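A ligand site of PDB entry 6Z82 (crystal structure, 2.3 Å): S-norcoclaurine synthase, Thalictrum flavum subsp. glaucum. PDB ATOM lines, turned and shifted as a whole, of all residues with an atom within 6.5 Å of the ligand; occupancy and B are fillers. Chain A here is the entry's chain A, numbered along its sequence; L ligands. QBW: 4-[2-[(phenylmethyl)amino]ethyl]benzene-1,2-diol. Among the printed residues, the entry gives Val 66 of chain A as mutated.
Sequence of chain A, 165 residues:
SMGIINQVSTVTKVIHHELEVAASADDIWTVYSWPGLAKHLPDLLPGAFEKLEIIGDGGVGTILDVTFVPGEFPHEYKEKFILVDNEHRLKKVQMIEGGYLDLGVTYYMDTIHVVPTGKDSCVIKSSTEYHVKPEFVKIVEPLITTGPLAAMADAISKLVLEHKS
O1 of the ligand lies within hydrogen-bond range of NZ of Lys 91 (2.7 Å).
OE2 of Glu 79 lies within salt-bridge range of N1 of the ligand (2.9 Å).
The backbone carbonyl oxygen (O) of Ile 112 lies within hydrogen-bond range of the backbone NH (N) of Lys 91 (2.8 Å).
NZ of Lys 91 sits at hydrogen-bond distance from O of Tyr 32 (3.0 Å).
The backbone NH (N) of Glu 79 sits at hydrogen-bond distance from the backbone carbonyl oxygen (O) of Leu 64.
O of Tyr 77 is in hydrogen-bond range of N of Val 66, at 2.8 Å.
O of Val 93 is in hydrogen-bond range of N of Asp 110.
Merely in contact with the ligand: Pro 148 (3.3 Å), Ile 112 (3.3 Å), Leu 64 (3.3 Å), Leu 37 (3.4 Å), Tyr 77 (3.5 Å), Met 152 (3.6 Å), Phe 68 (3.6 Å), Leu 45 (3.6 Å), Phe 81 (3.7 Å) and Val 93 (3.9 Å).
Hydrophobic or aromatic side chains within 4 Å of the ligand: Leu 37, Leu 45, Leu 64, Phe 68, Phe 81, Val 93, Ile 112, Pro 148 and Met 152.
12 residues have an atom within 4 Å of the ligand: Leu 37, Leu 45, Leu 64, Phe 68, Tyr 77, Glu 79, Phe 81, Lys 91, Val 93, Ile 112, Pro 148 and Met 152.
The nearest printed residue that does not touch the ligand is Leu 41 (4.1 Å).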
ATOM      1  N   TYR A  32       4.552  30.187 -27.469  1.00  0.00           N
ATOM      2  CA  TYR A  32       3.074  30.179 -27.679  1.00  0.00           C
ATOM      3  C   TYR A  32       2.642  28.933 -28.462  1.00  0.00           C
ATOM      4  O   TYR A  32       1.550  28.420 -28.178  1.00  0.00           O
ATOM      5  CB  TYR A  32       2.601  31.446 -28.391  1.00  0.00           C
ATOM      6  CG  TYR A  32       2.234  32.589 -27.460  1.00  0.00           C
ATOM      7  CD1 TYR A  32       1.115  32.534 -26.650  1.00  0.00           C
ATOM      8  CD2 TYR A  32       3.037  33.714 -27.399  1.00  0.00           C
ATOM      9  CE1 TYR A  32       0.778  33.578 -25.795  1.00  0.00           C
ATOM     10  CE2 TYR A  32       2.733  34.757 -26.538  1.00  0.00           C
ATOM     11  CZ  TYR A  32       1.599  34.695 -25.746  1.00  0.00           C
ATOM     12  OH  TYR A  32       1.310  35.729 -24.907  1.00  0.00           O
ATOM     13  N   LEU A  37       3.610  23.850 -23.821  1.00  0.00           N
ATOM     14  CA  LEU A  37       3.334  25.119 -23.099  1.00  0.00           C
ATOM     15  C   LEU A  37       2.258  24.875 -22.022  1.00  0.00           C
ATOM     16  O   LEU A  37       2.469  25.295 -20.847  1.00  0.00           O
ATOM     17  CB  LEU A  37       2.878  26.221 -24.071  1.00  0.00           C
ATOM     18  CG  LEU A  37       2.314  27.481 -23.397  1.00  0.00           C
ATOM     19  CD1 LEU A  37       3.380  28.179 -22.569  1.00  0.00           C
ATOM     20  CD2 LEU A  37       1.730  28.460 -24.419  1.00  0.00           C
ATOM     21  N   ALA A  38       1.138  24.254 -22.424  1.00  0.00           N
ATOM     22  CA  ALA A  38       0.000  23.881 -21.558  1.00  0.00           C
ATOM     23  C   ALA A  38       0.516  23.238 -20.267  1.00  0.00           C
ATOM     24  O   ALA A  38       0.220  23.795 -19.194  1.00  0.00           O
ATOM     25  CB  ALA A  38      -0.920  22.957 -22.323  1.00  0.00           C
ATOM     26  N   LEU A  41       2.148  25.447 -17.544  1.00  0.00           N
ATOM     27  CA  LEU A  41       1.353  26.668 -17.178  1.00  0.00           C
ATOM     28  C   LEU A  41       1.442  27.020 -15.694  1.00  0.00           C
ATOM     29  O   LEU A  41       1.634  28.200 -15.407  1.00  0.00           O
ATOM     30  CB  LEU A  41      -0.109  26.519 -17.630  1.00  0.00           C
ATOM     31  CG  LEU A  41      -0.429  27.204 -18.954  1.00  0.00           C
ATOM     32  CD1 LEU A  41      -1.886  27.020 -19.341  1.00  0.00           C
ATOM     33  CD2 LEU A  41      -0.067  28.687 -18.876  1.00  0.00           C
ATOM     34  N   LEU A  45       2.530  30.408 -13.928  1.00  0.00           N
ATOM     35  CA  LEU A  45       1.521  31.218 -13.183  1.00  0.00           C
ATOM     36  C   LEU A  45       1.023  30.451 -11.964  1.00  0.00           C
ATOM     37  O   LEU A  45      -0.058  29.853 -11.988  1.00  0.00           O
ATOM     38  CB  LEU A  45       0.371  31.543 -14.136  1.00  0.00           C
ATOM     39  CG  LEU A  45       0.681  32.636 -15.158  1.00  0.00           C
ATOM     40  CD1 LEU A  45      -0.317  32.597 -16.298  1.00  0.00           C
ATOM     41  CD2 LEU A  45       0.723  34.019 -14.484  1.00  0.00           C
ATOM     42  N   ALA A  48      -2.798  31.184  -9.561  1.00  0.00           N
ATOM     43  CA  ALA A  48      -3.938  31.172 -10.520  1.00  0.00           C
ATOM     44  C   ALA A  48      -4.761  29.892 -10.308  1.00  0.00           C
ATOM     45  O   ALA A  48      -5.933  30.001  -9.883  1.00  0.00           O
ATOM     46  CB  ALA A  48      -3.424  31.277 -11.937  1.00  0.00           C
ATOM     47  N   PHE A  49      -4.159  28.733 -10.591  1.00  0.00           N
ATOM     48  CA  PHE A  49      -4.868  27.444 -10.791  1.00  0.00           C
ATOM     49  C   PHE A  49      -4.963  26.662  -9.477  1.00  0.00           C
ATOM     50  O   PHE A  49      -3.945  26.499  -8.827  1.00  0.00           O
ATOM     51  CB  PHE A  49      -4.173  26.572 -11.838  1.00  0.00           C
ATOM     52  CG  PHE A  49      -3.924  27.301 -13.129  1.00  0.00           C
ATOM     53  CD1 PHE A  49      -4.983  27.896 -13.797  1.00  0.00           C
ATOM     54  CD2 PHE A  49      -2.647  27.432 -13.634  1.00  0.00           C
ATOM     55  CE1 PHE A  49      -4.763  28.600 -14.969  1.00  0.00           C
ATOM     56  CE2 PHE A  49      -2.429  28.135 -14.816  1.00  0.00           C
ATOM     57  CZ  PHE A  49      -3.493  28.713 -15.472  1.00  0.00           C
ATOM     58  N   LEU A  52      -5.288  21.719 -13.327  1.00  0.00           N
ATOM     59  CA  LEU A  52      -5.277  21.881 -14.808  1.00  0.00           C
ATOM     60  C   LEU A  52      -5.102  20.548 -15.549  1.00  0.00           C
ATOM     61  O   LEU A  52      -3.981  20.276 -15.969  1.00  0.00           O
ATOM     62  CB  LEU A  52      -4.164  22.860 -15.164  1.00  0.00           C
ATOM     63  CG  LEU A  52      -4.046  23.218 -16.651  1.00  0.00           C
ATOM     64  CD1 LEU A  52      -5.303  23.876 -17.175  1.00  0.00           C
ATOM     65  CD2 LEU A  52      -2.861  24.126 -16.877  1.00  0.00           C
ATOM     66  N   LEU A  64      -8.066  21.913 -22.409  1.00  0.00           N
ATOM     67  CA  LEU A  64      -7.639  22.252 -21.033  1.00  0.00           C
ATOM     68  C   LEU A  64      -8.899  22.321 -20.175  1.00  0.00           C
ATOM     69  O   LEU A  64      -9.779  23.110 -20.565  1.00  0.00           O
ATOM     70  CB  LEU A  64      -6.940  23.607 -21.062  1.00  0.00           C
ATOM     71  CG  LEU A  64      -5.444  23.597 -21.331  1.00  0.00           C
ATOM     72  CD1 LEU A  64      -5.102  22.715 -22.519  1.00  0.00           C
ATOM     73  CD2 LEU A  64      -4.930  25.000 -21.552  1.00  0.00           C
ATOM     74  N   VAL A  66      -9.703  23.755 -16.630  1.00  0.00           N
ATOM     75  CA  VAL A  66      -9.031  24.719 -15.710  1.00  0.00           C
ATOM     76  C   VAL A  66      -9.953  24.986 -14.516  1.00  0.00           C
ATOM     77  O   VAL A  66     -11.138  25.353 -14.736  1.00  0.00           O
ATOM     78  CB  VAL A  66      -8.668  26.034 -16.428  1.00  0.00           C
ATOM     79  CG1 VAL A  66      -7.531  26.760 -15.735  1.00  0.00           C
ATOM     80  CG2 VAL A  66      -8.346  25.825 -17.896  1.00  0.00           C
ATOM     81  N   PHE A  68      -9.996  27.269 -10.916  1.00  0.00           N
ATOM     82  CA  PHE A  68      -9.382  28.372 -10.134  1.00  0.00           C
ATOM     83  C   PHE A  68      -9.653  28.225  -8.617  1.00  0.00           C
ATOM     84  O   PHE A  68     -10.708  27.609  -8.216  1.00  0.00           O
ATOM     85  CB  PHE A  68      -9.838  29.723 -10.685  1.00  0.00           C
ATOM     86  CG  PHE A  68      -9.414  29.936 -12.110  1.00  0.00           C
ATOM     87  CD1 PHE A  68      -8.184  30.504 -12.410  1.00  0.00           C
ATOM     88  CD2 PHE A  68     -10.244  29.548 -13.157  1.00  0.00           C
ATOM     89  CE1 PHE A  68      -7.793  30.713 -13.728  1.00  0.00           C
ATOM     90  CE2 PHE A  68      -9.856  29.748 -14.474  1.00  0.00           C
ATOM     91  CZ  PHE A  68      -8.624  30.318 -14.755  1.00  0.00           C
ATOM     92  N   TYR A  77     -13.498  26.148 -16.210  1.00  0.00           N
ATOM     93  CA  TYR A  77     -13.937  26.075 -17.632  1.00  0.00           C
ATOM     94  C   TYR A  77     -12.944  25.246 -18.464  1.00  0.00           C
ATOM     95  O   TYR A  77     -11.802  25.039 -18.010  1.00  0.00           O
ATOM     96  CB  TYR A  77     -14.086  27.479 -18.223  1.00  0.00           C
ATOM     97  CG  TYR A  77     -12.856  28.340 -18.167  1.00  0.00           C
ATOM     98  CD1 TYR A  77     -11.757  28.090 -18.972  1.00  0.00           C
ATOM     99  CD2 TYR A  77     -12.843  29.472 -17.371  1.00  0.00           C
ATOM    100  CE1 TYR A  77     -10.635  28.901 -18.936  1.00  0.00           C
ATOM    101  CE2 TYR A  77     -11.727  30.296 -17.336  1.00  0.00           C
ATOM    102  CZ  TYR A  77     -10.617  30.014 -18.119  1.00  0.00           C
ATOM    103  OH  TYR A  77      -9.533  30.832 -18.058  1.00  0.00           O
ATOM    104  N   GLU A  79     -11.103  24.979 -22.241  1.00  0.00           N
ATOM    105  CA  GLU A  79     -10.539  25.709 -23.405  1.00  0.00           C
ATOM    106  C   GLU A  79     -10.082  24.652 -24.409  1.00  0.00           C
ATOM    107  O   GLU A  79      -9.857  23.532 -24.021  1.00  0.00           O
ATOM    108  CB  GLU A  79      -9.446  26.693 -22.955  1.00  0.00           C
ATOM    109  CG  GLU A  79     -10.069  27.955 -22.335  1.00  0.00           C
ATOM    110  CD  GLU A  79      -9.529  29.343 -22.659  1.00  0.00           C
ATOM    111  OE1 GLU A  79     -10.267  30.180 -23.298  1.00  0.00           O
ATOM    112  OE2 GLU A  79      -8.376  29.622 -22.237  1.00  0.00           O
ATOM    113  N   PHE A  81      -7.499  24.482 -28.030  1.00  0.00           N
ATOM    114  CA  PHE A  81      -6.631  25.051 -29.100  1.00  0.00           C
ATOM    115  C   PHE A  81      -7.317  24.765 -30.464  1.00  0.00           C
ATOM    116  O   PHE A  81      -7.586  23.577 -30.840  1.00  0.00           O
ATOM    117  CB  PHE A  81      -5.177  24.593 -28.961  1.00  0.00           C
ATOM    118  CG  PHE A  81      -4.555  24.772 -27.608  1.00  0.00           C
ATOM    119  CD1 PHE A  81      -5.104  25.629 -26.651  1.00  0.00           C
ATOM    120  CD2 PHE A  81      -3.359  24.125 -27.289  1.00  0.00           C
ATOM    121  CE1 PHE A  81      -4.494  25.806 -25.407  1.00  0.00           C
ATOM    122  CE2 PHE A  81      -2.753  24.300 -26.065  1.00  0.00           C
ATOM    123  CZ  PHE A  81      -3.322  25.132 -25.113  1.00  0.00           C
ATOM    124  N   LYS A  91      -2.440  32.258 -33.061  1.00  0.00           N
ATOM    125  CA  LYS A  91      -2.989  31.157 -32.236  1.00  0.00           C
ATOM    126  C   LYS A  91      -4.393  31.533 -31.816  1.00  0.00           C
ATOM    127  O   LYS A  91      -4.535  32.661 -31.343  1.00  0.00           O
ATOM    128  CB  LYS A  91      -2.130  30.998 -30.974  1.00  0.00           C
ATOM    129  CG  LYS A  91      -2.601  29.905 -30.050  1.00  0.00           C
ATOM    130  CD  LYS A  91      -1.664  29.621 -28.919  1.00  0.00           C
ATOM    131  CE  LYS A  91      -1.741  28.160 -28.533  1.00  0.00           C
ATOM    132  NZ  LYS A  91      -1.210  27.931 -27.175  1.00  0.00           N
ATOM    133  N   VAL A  93      -7.722  30.140 -29.264  1.00  0.00           N
ATOM    134  CA  VAL A  93      -8.114  29.302 -28.114  1.00  0.00           C
ATOM    135  C   VAL A  93      -9.558  29.680 -27.769  1.00  0.00           C
ATOM    136  O   VAL A  93      -9.846  30.849 -27.513  1.00  0.00           O
ATOM    137  CB  VAL A  93      -7.168  29.537 -26.946  1.00  0.00           C
ATOM    138  CG1 VAL A  93      -7.662  28.850 -25.685  1.00  0.00           C
ATOM    139  CG2 VAL A  93      -5.771  29.105 -27.329  1.00  0.00           C
ATOM    140  N   ASP A 110     -10.238  33.538 -27.622  1.00  0.00           N
ATOM    141  CA  ASP A 110      -8.952  34.258 -27.438  1.00  0.00           C
ATOM    142  C   ASP A 110      -8.115  34.159 -28.718  1.00  0.00           C
ATOM    143  O   ASP A 110      -8.017  33.069 -29.331  1.00  0.00           O
ATOM    144  CB  ASP A 110      -8.135  33.702 -26.260  1.00  0.00           C
ATOM    145  CG  ASP A 110      -8.783  33.937 -24.910  1.00  0.00           C
ATOM    146  OD1 ASP A 110      -9.335  35.053 -24.711  1.00  0.00           O
ATOM    147  OD2 ASP A 110      -8.780  32.981 -24.069  1.00  0.00           O
ATOM    148  N   ILE A 112      -4.114  35.293 -30.194  1.00  0.00           N
ATOM    149  CA  ILE A 112      -2.731  35.758 -29.896  1.00  0.00           C
ATOM    150  C   ILE A 112      -2.029  35.829 -31.235  1.00  0.00           C
ATOM    151  O   ILE A 112      -2.071  34.832 -31.989  1.00  0.00           O
ATOM    152  CB  ILE A 112      -2.051  34.855 -28.855  1.00  0.00           C
ATOM    153  CG1 ILE A 112      -2.669  35.073 -27.467  1.00  0.00           C
ATOM    154  CG2 ILE A 112      -0.557  35.120 -28.817  1.00  0.00           C
ATOM    155  CD1 ILE A 112      -3.104  33.809 -26.795  1.00  0.00           C
ATOM    156  N   GLY A 147      -6.826  40.546 -18.301  1.00  0.00           N
ATOM    157  CA  GLY A 147      -6.065  39.970 -17.175  1.00  0.00           C
ATOM    158  C   GLY A 147      -5.442  38.632 -17.524  1.00  0.00           C
ATOM    159  O   GLY A 147      -4.237  38.495 -17.432  1.00  0.00           O
ATOM    160  N   PRO A 148      -6.241  37.613 -17.921  1.00  0.00           N
ATOM    161  CA  PRO A 148      -5.708  36.296 -18.279  1.00  0.00           C
ATOM    162  C   PRO A 148      -4.651  36.273 -19.386  1.00  0.00           C
ATOM    163  O   PRO A 148      -3.647  35.564 -19.226  1.00  0.00           O
ATOM    164  CB  PRO A 148      -6.958  35.520 -18.737  1.00  0.00           C
ATOM    165  CG  PRO A 148      -8.090  36.173 -17.969  1.00  0.00           C
ATOM    166  CD  PRO A 148      -7.714  37.647 -17.922  1.00  0.00           C
ATOM    167  N   LEU A 149      -4.862  37.032 -20.460  1.00  0.00           N
ATOM    168  CA  LEU A 149      -3.950  37.073 -21.634  1.00  0.00           C
ATOM    169  C   LEU A 149      -2.742  37.980 -21.336  1.00  0.00           C
ATOM    170  O   LEU A 149      -1.655  37.628 -21.794  1.00  0.00           O
ATOM    171  CB  LEU A 149      -4.713  37.534 -22.881  1.00  0.00           C
ATOM    172  CG  LEU A 149      -5.679  36.508 -23.507  1.00  0.00           C
ATOM    173  CD1 LEU A 149      -6.291  37.061 -24.775  1.00  0.00           C
ATOM    174  CD2 LEU A 149      -5.007  35.164 -23.781  1.00  0.00           C
ATOM    175  N   ALA A 151      -1.415  38.252 -18.358  1.00  0.00           N
ATOM    176  CA  ALA A 151      -0.626  37.435 -17.404  1.00  0.00           C
ATOM    177  C   ALA A 151       0.176  36.410 -18.218  1.00  0.00           C
ATOM    178  O   ALA A 151       1.354  36.154 -17.856  1.00  0.00           O
ATOM    179  CB  ALA A 151      -1.511  36.795 -16.344  1.00  0.00           C
ATOM    180  N   MET A 152      -0.399  35.889 -19.309  1.00  0.00           N
ATOM    181  CA  MET A 152       0.295  34.952 -20.228  1.00  0.00           C
ATOM    182  C   MET A 152       1.394  35.677 -21.002  1.00  0.00           C
ATOM    183  O   MET A 152       2.478  35.117 -21.144  1.00  0.00           O
ATOM    184  CB  MET A 152      -0.678  34.353 -21.243  1.00  0.00           C
ATOM    185  CG  MET A 152      -1.495  33.244 -20.683  1.00  0.00           C
ATOM    186  SD  MET A 152      -1.281  31.780 -21.690  1.00  0.00           S
ATOM    187  CE  MET A 152       0.394  31.334 -21.239  1.00  0.00           C
ATOM    188  N   ILE A 156       5.339  34.706 -20.585  1.00  0.00           N
ATOM    189  CA  ILE A 156       6.087  34.180 -21.778  1.00  0.00           C
ATOM    190  C   ILE A 156       7.296  35.098 -22.020  1.00  0.00           C
ATOM    191  O   ILE A 156       8.466  34.557 -22.115  1.00  0.00           O
ATOM    192  CB  ILE A 156       5.158  34.005 -22.996  1.00  0.00           C
ATOM    193  CG1 ILE A 156       4.412  32.672 -22.880  1.00  0.00           C
ATOM    194  CG2 ILE A 156       5.903  34.096 -24.313  1.00  0.00           C
ATOM    195  CD1 ILE A 156       3.168  32.584 -23.736  1.00  0.00           C
HETATM  196  N1  QBW L   1      -6.266  30.416 -20.342  1.00  0.00           N
HETATM  197  C4  QBW L   1      -4.302  30.833 -24.005  1.00  0.00           C
HETATM  198  C5  QBW L   1      -4.978  30.234 -22.950  1.00  0.00           C
HETATM  199  C6  QBW L   1      -4.542  29.030 -22.402  1.00  0.00           C
HETATM  200  C7  QBW L   1      -5.278  28.313 -21.285  1.00  0.00           C
HETATM  201  C8  QBW L   1      -5.642  29.126 -20.046  1.00  0.00           C
HETATM  202  C10 QBW L   1      -5.178  31.931 -18.718  1.00  0.00           C
HETATM  203  C13 QBW L   1      -4.892  32.727 -16.068  1.00  0.00           C
HETATM  204  C15 QBW L   1      -3.980  32.458 -18.257  1.00  0.00           C
HETATM  205  C1  QBW L   1      -3.444  28.407 -22.986  1.00  0.00           C
HETATM  206  C2  QBW L   1      -2.761  28.992 -24.040  1.00  0.00           C
HETATM  207  C3  QBW L   1      -3.190  30.209 -24.560  1.00  0.00           C
HETATM  208  O1  QBW L   1      -1.658  28.373 -24.585  1.00  0.00           O
HETATM  209  O2  QBW L   1      -2.513  30.777 -25.602  1.00  0.00           O
HETATM  210  C9  QBW L   1      -5.347  31.529 -20.165  1.00  0.00           C
HETATM  211  C11 QBW L   1      -6.230  31.801 -17.819  1.00  0.00           C
HETATM  212  C12 QBW L   1      -6.086  32.203 -16.500  1.00  0.00           C
HETATM  213  C14 QBW L   1      -3.845  32.864 -16.937  1.00  0.00           C
